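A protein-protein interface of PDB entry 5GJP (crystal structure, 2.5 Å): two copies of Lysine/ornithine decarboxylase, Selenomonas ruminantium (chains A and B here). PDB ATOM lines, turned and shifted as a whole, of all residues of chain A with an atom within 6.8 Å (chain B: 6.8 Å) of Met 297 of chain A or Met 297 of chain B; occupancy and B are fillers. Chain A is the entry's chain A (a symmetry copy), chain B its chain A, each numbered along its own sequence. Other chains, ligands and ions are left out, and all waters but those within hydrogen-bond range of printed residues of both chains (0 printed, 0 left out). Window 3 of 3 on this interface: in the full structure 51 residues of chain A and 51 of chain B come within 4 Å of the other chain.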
ATOM      1  N   ILE A 289      19.531  11.418   1.557  1.00  0.00           N
ATOM      2  CA  ILE A 289      19.925  10.309   0.733  1.00  0.00           C
ATOM      3  C   ILE A 289      20.005   8.978   1.497  1.00  0.00           C
ATOM      4  O   ILE A 289      20.098   7.924   0.879  1.00  0.00           O
ATOM      5  CB  ILE A 289      21.291  10.628   0.042  1.00  0.00           C
ATOM      6  CG1 ILE A 289      21.388   9.964  -1.347  1.00  0.00           C
ATOM      7  CG2 ILE A 289      22.492  10.295   0.956  1.00  0.00           C
ATOM      8  CD1 ILE A 289      22.149  10.796  -2.365  1.00  0.00           C
ATOM      9  N   PHE A 293      15.274   9.646  -0.113  1.00  0.00           N
ATOM     10  CA  PHE A 293      16.029   9.970  -1.314  1.00  0.00           C
ATOM     11  C   PHE A 293      17.118   8.934  -1.643  1.00  0.00           C
ATOM     12  O   PHE A 293      17.908   9.165  -2.552  1.00  0.00           O
ATOM     13  CB  PHE A 293      16.659  11.348  -1.217  1.00  0.00           C
ATOM     14  CG  PHE A 293      15.670  12.465  -1.257  1.00  0.00           C
ATOM     15  CD1 PHE A 293      15.175  12.917  -2.485  1.00  0.00           C
ATOM     16  CD2 PHE A 293      15.267  13.097  -0.089  1.00  0.00           C
ATOM     17  CE1 PHE A 293      14.275  13.972  -2.536  1.00  0.00           C
ATOM     18  CE2 PHE A 293      14.354  14.140  -0.124  1.00  0.00           C
ATOM     19  CZ  PHE A 293      13.880  14.593  -1.354  1.00  0.00           C
ATOM     20  N   SER A 294      17.151   7.805  -0.929  1.00  0.00           N
ATOM     21  CA  SER A 294      18.027   6.657  -1.268  1.00  0.00           C
ATOM     22  C   SER A 294      17.845   6.132  -2.727  1.00  0.00           C
ATOM     23  O   SER A 294      18.759   5.502  -3.283  1.00  0.00           O
ATOM     24  CB  SER A 294      17.819   5.487  -0.271  1.00  0.00           C
ATOM     25  OG  SER A 294      16.450   5.109  -0.265  1.00  0.00           O
ATOM     26  N   GLY A 295      16.684   6.387  -3.317  1.00  0.00           N
ATOM     27  CA  GLY A 295      16.418   5.996  -4.687  1.00  0.00           C
ATOM     28  C   GLY A 295      17.277   6.701  -5.714  1.00  0.00           C
ATOM     29  O   GLY A 295      17.518   6.145  -6.766  1.00  0.00           O
ATOM     30  N   ILE A 296      17.764   7.904  -5.393  1.00  0.00           N
ATOM     31  CA  ILE A 296      18.840   8.560  -6.167  1.00  0.00           C
ATOM     32  C   ILE A 296      20.061   7.635  -6.367  1.00  0.00           C
ATOM     33  O   ILE A 296      20.676   7.652  -7.433  1.00  0.00           O
ATOM     34  CB  ILE A 296      19.276   9.880  -5.496  1.00  0.00           C
ATOM     35  CG1 ILE A 296      18.144  10.912  -5.556  1.00  0.00           C
ATOM     36  CG2 ILE A 296      20.540  10.454  -6.138  1.00  0.00           C
ATOM     37  CD1 ILE A 296      18.414  12.153  -4.723  1.00  0.00           C
ATOM     38  N   MET A 297      20.396   6.845  -5.344  1.00  0.00           N
ATOM     39  CA  MET A 297      21.568   5.944  -5.348  1.00  0.00           C
ATOM     40  C   MET A 297      21.302   4.557  -5.967  1.00  0.00           C
ATOM     41  O   MET A 297      22.027   4.106  -6.847  1.00  0.00           O
ATOM     42  CB  MET A 297      22.081   5.777  -3.916  1.00  0.00           C
ATOM     43  CG  MET A 297      23.573   5.602  -3.818  1.00  0.00           C
ATOM     44  SD  MET A 297      24.555   7.046  -4.293  1.00  0.00           S
ATOM     45  CE  MET A 297      23.649   8.405  -3.599  1.00  0.00           C
ATOM     46  N   TYR A 298      20.231   3.918  -5.524  1.00  0.00           N
ATOM     47  CA  TYR A 298      19.921   2.537  -5.851  1.00  0.00           C
ATOM     48  C   TYR A 298      18.971   2.353  -7.023  1.00  0.00           C
ATOM     49  O   TYR A 298      18.855   1.254  -7.558  1.00  0.00           O
ATOM     50  CB  TYR A 298      19.249   1.890  -4.636  1.00  0.00           C
ATOM     51  CG  TYR A 298      20.148   1.561  -3.481  1.00  0.00           C
ATOM     52  CD1 TYR A 298      21.012   0.472  -3.540  1.00  0.00           C
ATOM     53  CD2 TYR A 298      20.087   2.291  -2.291  1.00  0.00           C
ATOM     54  CE1 TYR A 298      21.810   0.144  -2.455  1.00  0.00           C
ATOM     55  CE2 TYR A 298      20.878   1.956  -1.201  1.00  0.00           C
ATOM     56  CZ  TYR A 298      21.737   0.886  -1.303  1.00  0.00           C
ATOM     57  OH  TYR A 298      22.532   0.555  -0.265  1.00  0.00           O
ATOM     58  N   ASP A 299      18.237   3.406  -7.359  1.00  0.00           N
ATOM     59  CA  ASP A 299      17.193   3.398  -8.386  1.00  0.00           C
ATOM     60  C   ASP A 299      17.454   4.440  -9.523  1.00  0.00           C
ATOM     61  O   ASP A 299      16.597   4.649 -10.362  1.00  0.00           O
ATOM     62  CB  ASP A 299      15.846   3.668  -7.662  1.00  0.00           C
ATOM     63  CG  ASP A 299      14.612   3.231  -8.469  1.00  0.00           C
ATOM     64  OD1 ASP A 299      14.657   2.168  -9.113  1.00  0.00           O
ATOM     65  OD2 ASP A 299      13.585   3.968  -8.477  1.00  0.00           O
ATOM     66  N   HIS A 300      18.630   5.086  -9.527  1.00  0.00           N
ATOM     67  CA  HIS A 300      19.025   6.153 -10.484  1.00  0.00           C
ATOM     68  C   HIS A 300      17.920   7.162 -10.798  1.00  0.00           C
ATOM     69  O   HIS A 300      17.687   7.530 -11.952  1.00  0.00           O
ATOM     70  CB  HIS A 300      19.554   5.525 -11.755  1.00  0.00           C
ATOM     71  CG  HIS A 300      20.670   4.564 -11.515  1.00  0.00           C
ATOM     72  ND1 HIS A 300      21.954   4.978 -11.221  1.00  0.00           N
ATOM     73  CD2 HIS A 300      20.688   3.209 -11.486  1.00  0.00           C
ATOM     74  CE1 HIS A 300      22.721   3.916 -11.048  1.00  0.00           C
ATOM     75  NE2 HIS A 300      21.978   2.832 -11.200  1.00  0.00           N
ATOM     76  N   TRP A 301      17.249   7.613  -9.749  1.00  0.00           N
ATOM     77  CA  TRP A 301      15.966   8.262  -9.913  1.00  0.00           C
ATOM     78  C   TRP A 301      16.098   9.723  -9.585  1.00  0.00           C
ATOM     79  O   TRP A 301      16.979  10.091  -8.839  1.00  0.00           O
ATOM     80  CB  TRP A 301      14.911   7.587  -9.024  1.00  0.00           C
ATOM     81  CG  TRP A 301      13.518   7.898  -9.475  1.00  0.00           C
ATOM     82  CD1 TRP A 301      12.760   8.952  -9.095  1.00  0.00           C
ATOM     83  CD2 TRP A 301      12.756   7.179 -10.440  1.00  0.00           C
ATOM     84  NE1 TRP A 301      11.545   8.925  -9.743  1.00  0.00           N
ATOM     85  CE2 TRP A 301      11.522   7.851 -10.581  1.00  0.00           C
ATOM     86  CE3 TRP A 301      12.994   6.040 -11.194  1.00  0.00           C
ATOM     87  CZ2 TRP A 301      10.541   7.427 -11.439  1.00  0.00           C
ATOM     88  CZ3 TRP A 301      12.026   5.607 -12.052  1.00  0.00           C
ATOM     89  CH2 TRP A 301      10.804   6.296 -12.172  1.00  0.00           C
ATOM     90  N   ILE A 326      28.213  12.965   0.944  1.00  0.00           N
ATOM     91  CA  ILE A 326      27.471  12.374  -0.160  1.00  0.00           C
ATOM     92  C   ILE A 326      25.981  12.821  -0.174  1.00  0.00           C
ATOM     93  O   ILE A 326      25.294  12.682  -1.190  1.00  0.00           O
ATOM     94  CB  ILE A 326      27.646  10.819  -0.140  1.00  0.00           C
ATOM     95  CG1 ILE A 326      27.416  10.215  -1.535  1.00  0.00           C
ATOM     96  CG2 ILE A 326      26.777  10.129   0.928  1.00  0.00           C
ATOM     97  CD1 ILE A 326      28.503   9.237  -1.905  1.00  0.00           C
ATOM     98  N   VAL A 328      23.752  14.962  -0.828  1.00  0.00           N
ATOM     99  CA  VAL A 328      23.365  16.087  -1.655  1.00  0.00           C
ATOM    100  C   VAL A 328      22.314  15.604  -2.628  1.00  0.00           C
ATOM    101  O   VAL A 328      22.539  14.646  -3.328  1.00  0.00           O
ATOM    102  CB  VAL A 328      24.571  16.607  -2.451  1.00  0.00           C
ATOM    103  CG1 VAL A 328      24.253  17.922  -3.117  1.00  0.00           C
ATOM    104  CG2 VAL A 328      25.783  16.738  -1.561  1.00  0.00           C
ATOM    105  N   ILE B 289      24.106  -5.578  -1.228  1.00  0.00           N
ATOM    106  CA  ILE B 289      24.313  -4.159  -1.310  1.00  0.00           C
ATOM    107  C   ILE B 289      23.241  -3.340  -0.574  1.00  0.00           C
ATOM    108  O   ILE B 289      23.419  -2.147  -0.367  1.00  0.00           O
ATOM    109  CB  ILE B 289      24.397  -3.728  -2.811  1.00  0.00           C
ATOM    110  CG1 ILE B 289      25.344  -2.525  -3.001  1.00  0.00           C
ATOM    111  CG2 ILE B 289      22.998  -3.497  -3.426  1.00  0.00           C
ATOM    112  CD1 ILE B 289      26.121  -2.562  -4.305  1.00  0.00           C
ATOM    113  N   PHE B 293      26.872  -4.577   2.697  1.00  0.00           N
ATOM    114  CA  PHE B 293      27.659  -4.104   1.568  1.00  0.00           C
ATOM    115  C   PHE B 293      27.161  -2.763   1.002  1.00  0.00           C
ATOM    116  O   PHE B 293      27.657  -2.329  -0.032  1.00  0.00           O
ATOM    117  CB  PHE B 293      27.702  -5.134   0.454  1.00  0.00           C
ATOM    118  CG  PHE B 293      28.493  -6.353   0.793  1.00  0.00           C
ATOM    119  CD1 PHE B 293      29.886  -6.342   0.663  1.00  0.00           C
ATOM    120  CD2 PHE B 293      27.859  -7.521   1.192  1.00  0.00           C
ATOM    121  CE1 PHE B 293      30.629  -7.478   0.950  1.00  0.00           C
ATOM    122  CE2 PHE B 293      28.591  -8.658   1.500  1.00  0.00           C
ATOM    123  CZ  PHE B 293      29.977  -8.640   1.352  1.00  0.00           C
ATOM    124  N   SER B 294      26.211  -2.107   1.676  1.00  0.00           N
ATOM    125  CA  SER B 294      25.783  -0.728   1.338  1.00  0.00           C
ATOM    126  C   SER B 294      26.951   0.307   1.306  1.00  0.00           C
ATOM    127  O   SER B 294      26.841   1.352   0.646  1.00  0.00           O
ATOM    128  CB  SER B 294      24.684  -0.233   2.315  1.00  0.00           C
ATOM    129  OG  SER B 294      25.167  -0.313   3.649  1.00  0.00           O
ATOM    130  N   GLY B 295      28.035   0.012   2.013  1.00  0.00           N
ATOM    131  CA  GLY B 295      29.203   0.869   2.019  1.00  0.00           C
ATOM    132  C   GLY B 295      29.907   0.972   0.683  1.00  0.00           C
ATOM    133  O   GLY B 295      30.536   1.977   0.422  1.00  0.00           O
ATOM    134  N   ILE B 296      29.771  -0.050  -0.168  1.00  0.00           N
ATOM    135  CA  ILE B 296      30.150   0.046  -1.595  1.00  0.00           C
ATOM    136  C   ILE B 296      29.518   1.276  -2.284  1.00  0.00           C
ATOM    137  O   ILE B 296      30.162   1.909  -3.121  1.00  0.00           O
ATOM    138  CB  ILE B 296      29.774  -1.243  -2.353  1.00  0.00           C
ATOM    139  CG1 ILE B 296      30.619  -2.423  -1.862  1.00  0.00           C
ATOM    140  CG2 ILE B 296      29.935  -1.081  -3.866  1.00  0.00           C
ATOM    141  CD1 ILE B 296      30.154  -3.765  -2.398  1.00  0.00           C
ATOM    142  N   MET B 297      28.271   1.594  -1.929  1.00  0.00           N
ATOM    143  CA  MET B 297      27.501   2.702  -2.531  1.00  0.00           C
ATOM    144  C   MET B 297      27.741   4.076  -1.872  1.00  0.00           C
ATOM    145  O   MET B 297      28.041   5.057  -2.542  1.00  0.00           O
ATOM    146  CB  MET B 297      26.009   2.365  -2.484  1.00  0.00           C
ATOM    147  CG  MET B 297      25.223   2.904  -3.649  1.00  0.00           C
ATOM    148  SD  MET B 297      25.619   2.172  -5.257  1.00  0.00           S
ATOM    149  CE  MET B 297      25.819   0.449  -4.884  1.00  0.00           C
ATOM    150  N   TYR B 298      27.645   4.112  -0.552  1.00  0.00           N
ATOM    151  CA  TYR B 298      27.657   5.339   0.225  1.00  0.00           C
ATOM    152  C   TYR B 298      29.016   5.735   0.779  1.00  0.00           C
ATOM    153  O   TYR B 298      29.202   6.870   1.208  1.00  0.00           O
ATOM    154  CB  TYR B 298      26.728   5.159   1.429  1.00  0.00           C
ATOM    155  CG  TYR B 298      25.257   5.192   1.140  1.00  0.00           C
ATOM    156  CD1 TYR B 298      24.612   6.395   0.867  1.00  0.00           C
ATOM    157  CD2 TYR B 298      24.483   4.031   1.212  1.00  0.00           C
ATOM    158  CE1 TYR B 298      23.245   6.429   0.643  1.00  0.00           C
ATOM    159  CE2 TYR B 298      23.112   4.066   0.998  1.00  0.00           C
ATOM    160  CZ  TYR B 298      22.512   5.270   0.709  1.00  0.00           C
ATOM    161  OH  TYR B 298      21.185   5.327   0.475  1.00  0.00           O
ATOM    162  N   ASP B 299      29.929   4.775   0.844  1.00  0.00           N
ATOM    163  CA  ASP B 299      31.257   4.929   1.442  1.00  0.00           C
ATOM    164  C   ASP B 299      32.413   4.619   0.435  1.00  0.00           C
ATOM    165  O   ASP B 299      33.564   4.562   0.833  1.00  0.00           O
ATOM    166  CB  ASP B 299      31.309   3.989   2.677  1.00  0.00           C
ATOM    167  CG  ASP B 299      32.407   4.356   3.688  1.00  0.00           C
ATOM    168  OD1 ASP B 299      32.625   5.556   3.933  1.00  0.00           O
ATOM    169  OD2 ASP B 299      33.076   3.435   4.236  1.00  0.00           O
ATOM    170  N   HIS B 300      32.091   4.415  -0.851  1.00  0.00           N
ATOM    171  CA  HIS B 300      33.044   4.044  -1.930  1.00  0.00           C
ATOM    172  C   HIS B 300      34.088   3.004  -1.523  1.00  0.00           C
ATOM    173  O   HIS B 300      35.278   3.131  -1.817  1.00  0.00           O
ATOM    174  CB  HIS B 300      33.713   5.291  -2.469  1.00  0.00           C
ATOM    175  CG  HIS B 300      32.741   6.326  -2.927  1.00  0.00           C
ATOM    176  ND1 HIS B 300      32.050   6.219  -4.118  1.00  0.00           N
ATOM    177  CD2 HIS B 300      32.313   7.471  -2.337  1.00  0.00           C
ATOM    178  CE1 HIS B 300      31.258   7.269  -4.254  1.00  0.00           C
ATOM    179  NE2 HIS B 300      31.397   8.040  -3.188  1.00  0.00           N
ATOM    180  N   TRP B 301      33.619   1.964  -0.850  1.00  0.00           N
ATOM    181  CA  TRP B 301      34.508   1.111  -0.090  1.00  0.00           C
ATOM    182  C   TRP B 301      34.596  -0.236  -0.752  1.00  0.00           C
ATOM    183  O   TRP B 301      33.684  -0.620  -1.449  1.00  0.00           O
ATOM    184  CB  TRP B 301      34.016   0.987   1.359  1.00  0.00           C
ATOM    185  CG  TRP B 301      35.099   0.515   2.278  1.00  0.00           C
ATOM    186  CD1 TRP B 301      35.413  -0.768   2.569  1.00  0.00           C
ATOM    187  CD2 TRP B 301      36.044   1.329   2.966  1.00  0.00           C
ATOM    188  NE1 TRP B 301      36.488  -0.814   3.430  1.00  0.00           N
ATOM    189  CE2 TRP B 301      36.898   0.461   3.682  1.00  0.00           C
ATOM    190  CE3 TRP B 301      36.250   2.697   3.049  1.00  0.00           C
ATOM    191  CZ2 TRP B 301      37.934   0.913   4.456  1.00  0.00           C
ATOM    192  CZ3 TRP B 301      37.278   3.161   3.818  1.00  0.00           C
ATOM    193  CH2 TRP B 301      38.114   2.273   4.520  1.00  0.00           C
ATOM    194  N   ILE B 326      21.286  -4.096  -9.473  1.00  0.00           N
ATOM    195  CA  ILE B 326      22.378  -3.325  -8.897  1.00  0.00           C
ATOM    196  C   ILE B 326      23.170  -4.131  -7.830  1.00  0.00           C
ATOM    197  O   ILE B 326      24.295  -3.767  -7.475  1.00  0.00           O
ATOM    198  CB  ILE B 326      21.831  -1.961  -8.356  1.00  0.00           C
ATOM    199  CG1 ILE B 326      22.943  -0.901  -8.294  1.00  0.00           C
ATOM    200  CG2 ILE B 326      21.101  -2.098  -7.007  1.00  0.00           C
ATOM    201  CD1 ILE B 326      22.499   0.409  -8.896  1.00  0.00           C
ATOM    202  N   VAL B 328      25.323  -6.311  -7.062  1.00  0.00           N
ATOM    203  CA  VAL B 328      26.524  -7.016  -7.465  1.00  0.00           C
ATOM    204  C   VAL B 328      27.671  -6.484  -6.636  1.00  0.00           C
ATOM    205  O   VAL B 328      27.890  -5.297  -6.607  1.00  0.00           O
ATOM    206  CB  VAL B 328      26.827  -6.756  -8.947  1.00  0.00           C
ATOM    207  CG1 VAL B 328      27.915  -7.674  -9.446  1.00  0.00           C
ATOM    208  CG2 VAL B 328      25.578  -6.907  -9.782  1.00  0.00           C
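The backbone carbonyl oxygen of Ile 289 of chain B is in hydrogen-bond range of the side-chain hydroxyl of Tyr 298 of chain A (2.8 Å). The side-chain hydroxyl of Tyr 298 of chain B lies within hydrogen-bond range of the backbone carbonyl oxygen of Ile 289 of chain A, 2.8 Å away.
The backbone carbonyl oxygen (O) of Ile 289 of chain B sits close to the backbone NH (N) of Ser 294 of chain B. N of His 300 of chain B is in hydrogen-bond range of O of Gly 295 of chain B. O of Ile 289 of chain A lies close to N of Ser 294 of chain A, at 3.5 Å. O of Gly 295 of chain A is in hydrogen-bond range of N of His 300 of chain A (3.2 Å).
Among the printed residues, merely in contact across the chains: Ser 294 of chain A with Tyr 298 of chain B (3.5 Å), Met 297 of chain A with Met 297 of chain B (3.2 Å), Tyr 298 of chain A with Ser 294 of chain B (3.5 Å), Tyr 298 of chain A with Tyr 298 of chain B (3.8 Å), Tyr 298 of chain A with Ile 326 of chain B (3.97 Å), His 300 of chain A with Ile 326 of chain B (3.4 Å), Ile 326 of chain A with Tyr 298 of chain B (3.97 Å) and Ile 326 of chain A with His 300 of chain B (3.4 Å).
Of chain B, only Met 297 comes within 4 Å of Met 297 of chain A. Of chain A, only Met 297 (3.2 Å) comes within 4 Å of Met 297 of chain B. Printed residues of chain A within 4 Å of Ile 289 of chain B: Tyr 298 (2.8 Å). Of the printed residues of chain B, His 300 of chain A touches Ile 326 (3.4 Å). Printed residues of chain B within 4 Å of Ile 289 of chain A: Tyr 298 (2.8 Å). Asp 299 of chain A touches none of the printed residues of chain B. The nearest residue of chain B that does not touch Met 297 of chain A is Ile 326 of chain B (4.3 Å).
Hydrophobic or aromatic side chains of chain A that line the printed part of chain B: Ile 289, Met 297, Tyr 298, His 300 and Ile 326. Hydrophobic or aromatic side chains of chain B that line the printed part of chain A: Ile 289, Met 297, Tyr 298, His 300 and Ile 326.
Ser 294 of chain A touches Tyr 298 of chain B, and with the chains exchanged Tyr 298 of chain A touches Ser 294 of chain B. Tyr 298 of chain A touches its own counterpart, Tyr 298 of chain B. Tyr 298 of chain A touches Ile 326 of chain B, and with the chains exchanged Ile 326 of chain A touches Tyr 298 of chain B. His 300 of chain A touches Ile 326 of chain B, and with the chains exchanged Ile 326 of chain A touches His 300 of chain B. Of the 10 pairs that touch across the chains among the printed residues, 10 have their exchanged pair printed and touching as well.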
